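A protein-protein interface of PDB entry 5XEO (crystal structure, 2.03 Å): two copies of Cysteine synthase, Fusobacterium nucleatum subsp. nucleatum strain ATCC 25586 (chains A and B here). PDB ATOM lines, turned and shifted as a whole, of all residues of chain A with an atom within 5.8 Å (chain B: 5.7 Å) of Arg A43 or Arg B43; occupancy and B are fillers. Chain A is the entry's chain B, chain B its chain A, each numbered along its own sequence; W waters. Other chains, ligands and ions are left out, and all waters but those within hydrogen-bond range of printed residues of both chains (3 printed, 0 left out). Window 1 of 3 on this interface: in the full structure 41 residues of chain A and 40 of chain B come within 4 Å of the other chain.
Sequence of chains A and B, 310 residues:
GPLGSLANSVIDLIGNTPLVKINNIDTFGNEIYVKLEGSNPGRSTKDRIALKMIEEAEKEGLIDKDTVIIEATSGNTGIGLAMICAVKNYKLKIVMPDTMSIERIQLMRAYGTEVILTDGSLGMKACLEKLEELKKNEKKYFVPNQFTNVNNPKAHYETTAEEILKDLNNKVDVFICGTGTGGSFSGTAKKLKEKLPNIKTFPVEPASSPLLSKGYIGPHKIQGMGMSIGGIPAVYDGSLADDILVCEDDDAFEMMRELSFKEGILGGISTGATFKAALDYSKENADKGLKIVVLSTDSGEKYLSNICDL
Printed residues of chain B within 4 Å of Gly A38: Arg B43.
Of the printed residues of chain B, Arg A43 touches Gly B38, Arg B43, Ser B299 and Glu B301.
Ser A44 touches none of the printed residues of chain B.
Printed residues of chain B within 4 Å of Glu A301: Arg B43 (3.3 Å).
Of the printed residues of chain A, Gly B38 touches Arg A43.
Of the printed residues of chain A, Ser B299 touches Arg A43.
Of the printed residues of chain A, Glu B301 touches Arg A43 (3.5 Å).
The nearest printed residue of chain B that does not touch Glu A301 is Glu B301 (4.7 Å).
The guanidinium group (NH1) of Arg B43 lies close to the backbone carbonyl oxygen (O) of Gly B38 (3.5 Å).
The backbone carbonyl oxygen (O) of Arg A43 sits at hydrogen-bond distance from the backbone NH (N) of Ser A299, at 3.3 Å.
NH1 of Arg A43 sits at hydrogen-bond distance from O of Asn A40, 3.1 Å away.
O of Asn B40 lies close to NH1 of Arg B43 (3.5 Å).
The backbone NH of Ser B299 is in hydrogen-bond range of the backbone carbonyl oxygen of Arg B43 (3.2 Å).
The side-chain hydroxyl (OG) of Ser A299 is in hydrogen-bond range of the side-chain carboxylate (OE1) of Glu A301 (2.5 Å).
Gly A38 touches Arg B43, and with the chains exchanged Arg A43 touches Gly B38.
Arg A43 touches its own counterpart, Arg B43.
Arg A43 touches Ser B299, and with the chains exchanged Ser A299 touches Arg B43.
Arg A43 touches Glu B301, and with the chains exchanged Glu A301 touches Arg B43.
Positions printed for both chains: 37, 38, 39, 40, 41, 42, 43, 44, 45, 47, 76, 297, 298, 299, 301 and 302.
NH2 of Arg B43 is in hydrogen-bond range of O of Gly A38.
The side-chain carboxylate (OE2) of Glu B301 is in salt-bridge range of the guanidinium group (NE) of Arg A43, 3.5 Å away.
The backbone carbonyl oxygen (O) of Gly B38 lies within hydrogen-bond range of the guanidinium group (NH2) of Arg A43, at 3.1 Å.
The guanidinium group of Arg B43 is in salt-bridge range of the side-chain carboxylate of Glu A301 (3.3 Å).
Water W2 lies within hydrogen-bond range of O of Ser A39 (2.8 Å), O of Ser B39 (3.1 Å) and NH1 of Arg B43 (3.4 Å).
Water W3 lies within hydrogen-bond range of the side-chain hydroxyl of Ser A39 (2.9 Å) and the guanidinium group of Arg B43 (3.5 Å).
Water W1 bridges the side-chain hydroxyl of Ser B39 (2.9 Å) and the guanidinium group of Arg A43 (3.5 Å).
Arg B43 touches Arg A43.
Arg A43 touches Ser B299.
NH2 of Arg B43 touches CB of Ser A299, at 3.8 Å.
Of the 16 printed residues of chain B, 4 touch a printed residue of chain A.
Of the 17 printed residues of chain A, 4 touch a printed residue of chain B.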
ATOM      1  N   GLU A  37      26.888   0.693  23.748  1.00  0.00           N
ATOM      2  CA  GLU A  37      27.714   0.405  22.576  1.00  0.00           C
ATOM      3  C   GLU A  37      27.081   0.852  21.254  1.00  0.00           C
ATOM      4  O   GLU A  37      27.781   1.010  20.257  1.00  0.00           O
ATOM      5  CB  GLU A  37      28.099  -1.070  22.547  1.00  0.00           C
ATOM      6  CG  GLU A  37      28.910  -1.472  23.772  1.00  0.00           C
ATOM      7  CD  GLU A  37      30.280  -0.859  23.727  1.00  0.00           C
ATOM      8  OE1 GLU A  37      31.007  -1.151  22.726  1.00  0.00           O
ATOM      9  OE2 GLU A  37      30.624  -0.098  24.650  1.00  0.00           O
ATOM     10  N   GLY A  38      25.774   1.120  21.282  1.00  0.00           N
ATOM     11  CA  GLY A  38      25.111   1.892  20.255  1.00  0.00           C
ATOM     12  C   GLY A  38      25.664   3.268  19.946  1.00  0.00           C
ATOM     13  O   GLY A  38      25.413   3.772  18.847  1.00  0.00           O
ATOM     14  N   SER A  39      26.429   3.854  20.865  1.00  0.00           N
ATOM     15  CA  SER A  39      27.096   5.123  20.636  1.00  0.00           C
ATOM     16  C   SER A  39      28.324   5.068  19.784  1.00  0.00           C
ATOM     17  O   SER A  39      28.814   6.124  19.394  1.00  0.00           O
ATOM     18  CB  SER A  39      27.510   5.789  21.963  1.00  0.00           C
ATOM     19  OG  SER A  39      26.355   5.875  22.759  1.00  0.00           O
ATOM     20  N   ASN A  40      28.858   3.866  19.550  1.00  0.00           N
ATOM     21  CA  ASN A  40      29.927   3.690  18.581  1.00  0.00           C
ATOM     22  C   ASN A  40      29.456   4.215  17.210  1.00  0.00           C
ATOM     23  O   ASN A  40      28.256   4.117  16.871  1.00  0.00           O
ATOM     24  CB  ASN A  40      30.321   2.204  18.452  1.00  0.00           C
ATOM     25  CG  ASN A  40      31.200   1.728  19.575  1.00  0.00           C
ATOM     26  OD1 ASN A  40      32.300   2.231  19.771  1.00  0.00           O
ATOM     27  ND2 ASN A  40      30.708   0.736  20.351  1.00  0.00           N
ATOM     28  N   PRO A  41      30.406   4.686  16.379  1.00  0.00           N
ATOM     29  CA  PRO A  41      30.032   5.253  15.070  1.00  0.00           C
ATOM     30  C   PRO A  41      29.274   4.268  14.163  1.00  0.00           C
ATOM     31  O   PRO A  41      28.335   4.660  13.483  1.00  0.00           O
ATOM     32  CB  PRO A  41      31.376   5.741  14.484  1.00  0.00           C
ATOM     33  CG  PRO A  41      32.461   5.118  15.321  1.00  0.00           C
ATOM     34  CD  PRO A  41      31.841   4.832  16.673  1.00  0.00           C
ATOM     35  N   GLY A  42      29.605   2.982  14.224  1.00  0.00           N
ATOM     36  CA  GLY A  42      28.860   1.956  13.531  1.00  0.00           C
ATOM     37  C   GLY A  42      27.624   1.426  14.227  1.00  0.00           C
ATOM     38  O   GLY A  42      26.969   0.518  13.719  1.00  0.00           O
ATOM     39  N   ARG A  43      27.318   1.995  15.397  1.00  0.00           N
ATOM     40  CA  ARG A  43      26.091   1.742  16.154  1.00  0.00           C
ATOM     41  C   ARG A  43      26.057   0.373  16.850  1.00  0.00           C
ATOM     42  O   ARG A  43      25.005  -0.052  17.290  1.00  0.00           O
ATOM     43  CB  ARG A  43      24.828   1.972  15.306  1.00  0.00           C
ATOM     44  CG  ARG A  43      24.743   3.354  14.681  1.00  0.00           C
ATOM     45  CD  ARG A  43      24.442   4.357  15.748  1.00  0.00           C
ATOM     46  NE  ARG A  43      24.385   5.730  15.277  1.00  0.00           N
ATOM     47  CZ  ARG A  43      25.220   6.729  15.583  1.00  0.00           C
ATOM     48  NH1 ARG A  43      26.287   6.521  16.390  1.00  0.00           N
ATOM     49  NH2 ARG A  43      24.990   7.950  15.099  1.00  0.00           N
ATOM     50  N   SER A  44      27.214  -0.265  17.002  1.00  0.00           N
ATOM     51  CA  SER A  44      27.298  -1.517  17.778  1.00  0.00           C
ATOM     52  C   SER A  44      28.679  -1.688  18.367  1.00  0.00           C
ATOM     53  O   SER A  44      29.665  -1.053  17.921  1.00  0.00           O
ATOM     54  CB  SER A  44      26.950  -2.744  16.941  1.00  0.00           C
ATOM     55  OG  SER A  44      28.110  -3.298  16.339  1.00  0.00           O
ATOM     56  N   THR A  45      28.744  -2.570  19.378  1.00  0.00           N
ATOM     57  CA  THR A  45      30.001  -2.938  19.958  1.00  0.00           C
ATOM     58  C   THR A  45      30.999  -3.535  18.931  1.00  0.00           C
ATOM     59  O   THR A  45      32.207  -3.521  19.170  1.00  0.00           O
ATOM     60  CB  THR A  45      29.812  -3.925  21.142  1.00  0.00           C
ATOM     61  OG1 THR A  45      30.893  -3.746  22.029  1.00  0.00           O
ATOM     62  CG2 THR A  45      29.746  -5.375  20.722  1.00  0.00           C
ATOM     63  N   ASP A  47      32.092  -2.559  16.139  1.00  0.00           N
ATOM     64  CA  ASP A  47      33.124  -1.614  15.705  1.00  0.00           C
ATOM     65  C   ASP A  47      34.471  -1.959  16.365  1.00  0.00           C
ATOM     66  O   ASP A  47      35.531  -1.867  15.733  1.00  0.00           O
ATOM     67  CB  ASP A  47      32.804  -0.163  16.104  1.00  0.00           C
ATOM     68  CG  ASP A  47      31.663   0.476  15.312  1.00  0.00           C
ATOM     69  OD1 ASP A  47      31.012  -0.215  14.515  1.00  0.00           O
ATOM     70  OD2 ASP A  47      31.421   1.674  15.505  1.00  0.00           O
ATOM     71  N   ASN A  76      25.954  -6.978  12.598  1.00  0.00           N
ATOM     72  CA  ASN A  76      26.701  -5.865  13.166  1.00  0.00           C
ATOM     73  C   ASN A  76      28.177  -5.954  12.920  1.00  0.00           C
ATOM     74  O   ASN A  76      28.827  -4.913  12.705  1.00  0.00           O
ATOM     75  CB  ASN A  76      26.379  -5.634  14.650  1.00  0.00           C
ATOM     76  CG  ASN A  76      25.052  -4.935  14.833  1.00  0.00           C
ATOM     77  OD1 ASN A  76      24.723  -4.020  14.062  1.00  0.00           O
ATOM     78  ND2 ASN A  76      24.265  -5.372  15.817  1.00  0.00           N
ATOM     79  N   ILE A  79      28.564  -4.518   9.591  1.00  0.00           N
ATOM     80  CA  ILE A  79      28.487  -3.035   9.658  1.00  0.00           C
ATOM     81  C   ILE A  79      29.743  -2.371  10.170  1.00  0.00           C
ATOM     82  O   ILE A  79      30.255  -1.381   9.590  1.00  0.00           O
ATOM     83  CB  ILE A  79      27.255  -2.586  10.500  1.00  0.00           C
ATOM     84  CG1 ILE A  79      25.980  -3.028   9.798  1.00  0.00           C
ATOM     85  CG2 ILE A  79      27.270  -1.058  10.700  1.00  0.00           C
ATOM     86  CD1 ILE A  79      24.734  -3.024  10.683  1.00  0.00           C
ATOM     87  N   THR A 297      24.454  -3.888  23.391  1.00  0.00           N
ATOM     88  CA  THR A 297      25.348  -4.190  22.269  1.00  0.00           C
ATOM     89  C   THR A 297      25.114  -3.279  21.066  1.00  0.00           C
ATOM     90  O   THR A 297      26.066  -2.922  20.400  1.00  0.00           O
ATOM     91  CB  THR A 297      25.249  -5.671  21.857  1.00  0.00           C
ATOM     92  OG1 THR A 297      25.584  -6.458  22.979  1.00  0.00           O
ATOM     93  CG2 THR A 297      26.197  -6.033  20.737  1.00  0.00           C
ATOM     94  N   ASP A 298      23.860  -2.905  20.794  1.00  0.00           N
ATOM     95  CA  ASP A 298      23.606  -1.978  19.714  1.00  0.00           C
ATOM     96  C   ASP A 298      22.416  -1.059  19.953  1.00  0.00           C
ATOM     97  O   ASP A 298      21.659  -1.246  20.881  1.00  0.00           O
ATOM     98  CB  ASP A 298      23.547  -2.723  18.348  1.00  0.00           C
ATOM     99  CG  ASP A 298      22.231  -3.423  18.043  1.00  0.00           C
ATOM    100  OD1 ASP A 298      21.407  -3.671  18.978  1.00  0.00           O
ATOM    101  OD2 ASP A 298      22.044  -3.826  16.878  1.00  0.00           O
ATOM    102  N   SER A 299      22.286  -0.047  19.121  1.00  0.00           N
ATOM    103  CA  SER A 299      21.153   0.871  19.247  1.00  0.00           C
ATOM    104  C   SER A 299      19.921   0.261  18.546  1.00  0.00           C
ATOM    105  O   SER A 299      20.043  -0.663  17.746  1.00  0.00           O
ATOM    106  CB  SER A 299      21.511   2.236  18.661  1.00  0.00           C
ATOM    107  OG  SER A 299      21.561   2.084  17.282  1.00  0.00           O
ATOM    108  N   GLU A 301      17.500   1.723  16.560  1.00  0.00           N
ATOM    109  CA  GLU A 301      16.925   2.356  15.366  1.00  0.00           C
ATOM    110  C   GLU A 301      16.761   1.352  14.236  1.00  0.00           C
ATOM    111  O   GLU A 301      15.796   1.423  13.494  1.00  0.00           O
ATOM    112  CB  GLU A 301      17.760   3.529  14.853  1.00  0.00           C
ATOM    113  CG  GLU A 301      17.874   4.706  15.810  1.00  0.00           C
ATOM    114  CD  GLU A 301      19.123   4.685  16.697  1.00  0.00           C
ATOM    115  OE1 GLU A 301      20.096   3.953  16.384  1.00  0.00           O
ATOM    116  OE2 GLU A 301      19.130   5.424  17.714  1.00  0.00           O
ATOM    117  N   LYS A 302      17.662   0.373  14.152  1.00  0.00           N
ATOM    118  CA  LYS A 302      17.609  -0.586  13.055  1.00  0.00           C
ATOM    119  C   LYS A 302      16.533  -1.672  13.219  1.00  0.00           C
ATOM    120  O   LYS A 302      16.449  -2.554  12.376  1.00  0.00           O
ATOM    121  CB  LYS A 302      19.008  -1.199  12.802  1.00  0.00           C
ATOM    122  CG  LYS A 302      19.509  -2.243  13.799  1.00  0.00           C
ATOM    123  CD  LYS A 302      20.851  -2.794  13.327  1.00  0.00           C
ATOM    124  CE  LYS A 302      22.126  -2.422  14.066  1.00  0.00           C
ATOM    125  NZ  LYS A 302      22.073  -1.206  14.927  1.00  0.00           N
ATOM    126  N   GLU B  37      26.547  15.897  14.850  1.00  0.00           N
ATOM    127  CA  GLU B  37      25.408  15.975  15.764  1.00  0.00           C
ATOM    128  C   GLU B  37      24.555  14.689  15.814  1.00  0.00           C
ATOM    129  O   GLU B  37      23.773  14.498  16.766  1.00  0.00           O
ATOM    130  CB  GLU B  37      24.545  17.189  15.461  1.00  0.00           C
ATOM    131  CG  GLU B  37      25.295  18.480  15.577  1.00  0.00           C
ATOM    132  CD  GLU B  37      25.575  18.842  17.005  1.00  0.00           C
ATOM    133  OE1 GLU B  37      24.584  18.935  17.780  1.00  0.00           O
ATOM    134  OE2 GLU B  37      26.768  19.032  17.342  1.00  0.00           O
ATOM    135  N   GLY B  38      24.763  13.781  14.857  1.00  0.00           N
ATOM    136  CA  GLY B  38      24.261  12.440  14.943  1.00  0.00           C
ATOM    137  C   GLY B  38      24.722  11.611  16.128  1.00  0.00           C
ATOM    138  O   GLY B  38      24.083  10.616  16.465  1.00  0.00           O
ATOM    139  N   SER B  39      25.830  12.025  16.747  1.00  0.00           N
ATOM    140  CA  SER B  39      26.319  11.488  17.992  1.00  0.00           C
ATOM    141  C   SER B  39      25.427  11.720  19.195  1.00  0.00           C
ATOM    142  O   SER B  39      25.584  11.009  20.169  1.00  0.00           O
ATOM    143  CB  SER B  39      27.656  12.119  18.351  1.00  0.00           C
ATOM    144  OG  SER B  39      28.616  11.672  17.429  1.00  0.00           O
ATOM    145  N   ASN B  40      24.571  12.750  19.153  1.00  0.00           N
ATOM    146  CA  ASN B  40      23.604  12.978  20.225  1.00  0.00           C
ATOM    147  C   ASN B  40      22.758  11.728  20.420  1.00  0.00           C
ATOM    148  O   ASN B  40      22.519  11.005  19.464  1.00  0.00           O
ATOM    149  CB  ASN B  40      22.720  14.169  19.909  1.00  0.00           C
ATOM    150  CG  ASN B  40      23.444  15.483  20.096  1.00  0.00           C
ATOM    151  OD1 ASN B  40      23.891  15.782  21.186  1.00  0.00           O
ATOM    152  ND2 ASN B  40      23.601  16.244  19.029  1.00  0.00           N
ATOM    153  N   PRO B  41      22.249  11.493  21.640  1.00  0.00           N
ATOM    154  CA  PRO B  41      21.509  10.242  21.902  1.00  0.00           C
ATOM    155  C   PRO B  41      20.196  10.146  21.133  1.00  0.00           C
ATOM    156  O   PRO B  41      19.768   9.057  20.837  1.00  0.00           O
ATOM    157  CB  PRO B  41      21.262  10.277  23.433  1.00  0.00           C
ATOM    158  CG  PRO B  41      21.399  11.744  23.789  1.00  0.00           C
ATOM    159  CD  PRO B  41      22.410  12.308  22.853  1.00  0.00           C
ATOM    160  N   GLY B  42      19.568  11.266  20.775  1.00  0.00           N
ATOM    161  CA  GLY B  42      18.415  11.225  19.878  1.00  0.00           C
ATOM    162  C   GLY B  42      18.807  11.319  18.410  1.00  0.00           C
ATOM    163  O   GLY B  42      17.930  11.441  17.542  1.00  0.00           O
ATOM    164  N   ARG B  43      20.119  11.316  18.140  1.00  0.00           N
ATOM    165  CA  ARG B  43      20.682  11.249  16.771  1.00  0.00           C
ATOM    166  C   ARG B  43      20.577  12.524  15.929  1.00  0.00           C
ATOM    167  O   ARG B  43      20.738  12.479  14.694  1.00  0.00           O
ATOM    168  CB  ARG B  43      20.124  10.054  15.964  1.00  0.00           C
ATOM    169  CG  ARG B  43      20.250   8.680  16.611  1.00  0.00           C
ATOM    170  CD  ARG B  43      21.680   8.376  16.847  1.00  0.00           C
ATOM    171  NE  ARG B  43      21.934   7.112  17.544  1.00  0.00           N
ATOM    172  CZ  ARG B  43      22.970   6.899  18.355  1.00  0.00           C
ATOM    173  NH1 ARG B  43      23.846   7.911  18.645  1.00  0.00           N
ATOM    174  NH2 ARG B  43      23.122   5.713  18.916  1.00  0.00           N
ATOM    175  N   SER B  44      20.327  13.644  16.582  1.00  0.00           N
ATOM    176  CA  SER B  44      20.346  14.933  15.907  1.00  0.00           C
ATOM    177  C   SER B  44      20.677  16.059  16.850  1.00  0.00           C
ATOM    178  O   SER B  44      20.617  15.902  18.070  1.00  0.00           O
ATOM    179  CB  SER B  44      18.997  15.212  15.205  1.00  0.00           C
ATOM    180  OG  SER B  44      18.053  15.876  16.051  1.00  0.00           O
ATOM    181  N   THR B  45      20.986  17.218  16.252  1.00  0.00           N
ATOM    182  CA  THR B  45      21.256  18.417  16.996  1.00  0.00           C
ATOM    183  C   THR B  45      20.019  18.890  17.775  1.00  0.00           C
ATOM    184  O   THR B  45      20.152  19.640  18.727  1.00  0.00           O
ATOM    185  CB  THR B  45      21.761  19.562  16.071  1.00  0.00           C
ATOM    186  OG1 THR B  45      22.631  20.383  16.803  1.00  0.00           O
ATOM    187  CG2 THR B  45      20.627  20.432  15.488  1.00  0.00           C
ATOM    188  N   ASP B  47      18.240  17.464  19.858  1.00  0.00           N
ATOM    189  CA  ASP B  47      18.308  17.120  21.292  1.00  0.00           C
ATOM    190  C   ASP B  47      18.702  18.346  22.122  1.00  0.00           C
ATOM    191  O   ASP B  47      18.231  18.522  23.261  1.00  0.00           O
ATOM    192  CB  ASP B  47      19.397  16.088  21.573  1.00  0.00           C
ATOM    193  CG  ASP B  47      19.086  14.686  21.086  1.00  0.00           C
ATOM    194  OD1 ASP B  47      18.011  14.464  20.471  1.00  0.00           O
ATOM    195  OD2 ASP B  47      19.922  13.793  21.339  1.00  0.00           O
ATOM    196  N   ASN B  76      13.077  15.841  13.509  1.00  0.00           N
ATOM    197  CA  ASN B  76      13.979  15.545  14.572  1.00  0.00           C
ATOM    198  C   ASN B  76      13.634  16.227  15.885  1.00  0.00           C
ATOM    199  O   ASN B  76      13.942  15.681  16.952  1.00  0.00           O
ATOM    200  CB  ASN B  76      15.393  15.900  14.185  1.00  0.00           C
ATOM    201  CG  ASN B  76      16.016  14.839  13.280  1.00  0.00           C
ATOM    202  OD1 ASN B  76      15.829  13.632  13.521  1.00  0.00           O
ATOM    203  ND2 ASN B  76      16.755  15.268  12.270  1.00  0.00           N
ATOM    204  N   THR B 297      23.835  17.704  10.901  1.00  0.00           N
ATOM    205  CA  THR B 297      22.711  17.868  11.806  1.00  0.00           C
ATOM    206  C   THR B 297      22.153  16.557  12.355  1.00  0.00           C
ATOM    207  O   THR B 297      21.785  16.533  13.516  1.00  0.00           O
ATOM    208  CB  THR B 297      21.615  18.772  11.200  1.00  0.00           C
ATOM    209  OG1 THR B 297      22.220  20.052  10.916  1.00  0.00           O
ATOM    210  CG2 THR B 297      20.456  18.977  12.170  1.00  0.00           C
ATOM    211  N   ASP B 298      22.118  15.482  11.565  1.00  0.00           N
ATOM    212  CA  ASP B 298      21.695  14.187  12.105  1.00  0.00           C
ATOM    213  C   ASP B 298      22.431  13.066  11.414  1.00  0.00           C
ATOM    214  O   ASP B 298      23.136  13.290  10.436  1.00  0.00           O
ATOM    215  CB  ASP B 298      20.160  14.003  12.065  1.00  0.00           C
ATOM    216  CG  ASP B 298      19.583  13.768  10.695  1.00  0.00           C
ATOM    217  OD1 ASP B 298      20.262  14.069   9.687  1.00  0.00           O
ATOM    218  OD2 ASP B 298      18.407  13.350  10.625  1.00  0.00           O
ATOM    219  N   SER B 299      22.249  11.863  11.928  1.00  0.00           N
ATOM    220  CA  SER B 299      22.906  10.714  11.358  1.00  0.00           C
ATOM    221  C   SER B 299      21.981  10.213  10.284  1.00  0.00           C
ATOM    222  O   SER B 299      20.824  10.599  10.233  1.00  0.00           O
ATOM    223  CB  SER B 299      23.190   9.647  12.418  1.00  0.00           C
ATOM    224  OG  SER B 299      21.996   9.177  12.945  1.00  0.00           O
ATOM    225  N   GLU B 301      20.959   7.037   9.385  1.00  0.00           N
ATOM    226  CA  GLU B 301      20.282   5.722   9.448  1.00  0.00           C
ATOM    227  C   GLU B 301      18.812   5.808   9.052  1.00  0.00           C
ATOM    228  O   GLU B 301      18.328   4.992   8.282  1.00  0.00           O
ATOM    229  CB  GLU B 301      20.333   5.099  10.850  1.00  0.00           C
ATOM    230  CG  GLU B 301      21.708   4.761  11.365  1.00  0.00           C
ATOM    231  CD  GLU B 301      22.396   5.899  12.098  1.00  0.00           C
ATOM    232  OE1 GLU B 301      21.728   6.619  12.879  1.00  0.00           O
ATOM    233  OE2 GLU B 301      23.635   6.043  11.900  1.00  0.00           O
ATOM    234  N   LYS B 302      18.117   6.812   9.582  1.00  0.00           N
ATOM    235  CA  LYS B 302      16.676   6.947   9.376  1.00  0.00           C
ATOM    236  C   LYS B 302      16.270   7.171   7.894  1.00  0.00           C
ATOM    237  O   LYS B 302      15.120   6.997   7.589  1.00  0.00           O
ATOM    238  CB  LYS B 302      16.091   8.070  10.275  1.00  0.00           C
ATOM    239  CG  LYS B 302      16.457   9.494   9.838  1.00  0.00           C
ATOM    240  CD  LYS B 302      15.830  10.626  10.675  1.00  0.00           C
ATOM    241  CE  LYS B 302      16.277  10.644  12.136  1.00  0.00           C
ATOM    242  NZ  LYS B 302      17.742  10.948  12.270  1.00  0.00           N
HETATM  243  O   HOH W   1      28.174   9.360  15.735  1.00  0.00           O
HETATM  244  O   HOH W   2      27.082   8.352  19.465  1.00  0.00           O
HETATM  245  O   HOH W   3      24.171   7.585  22.104  1.00  0.00           O
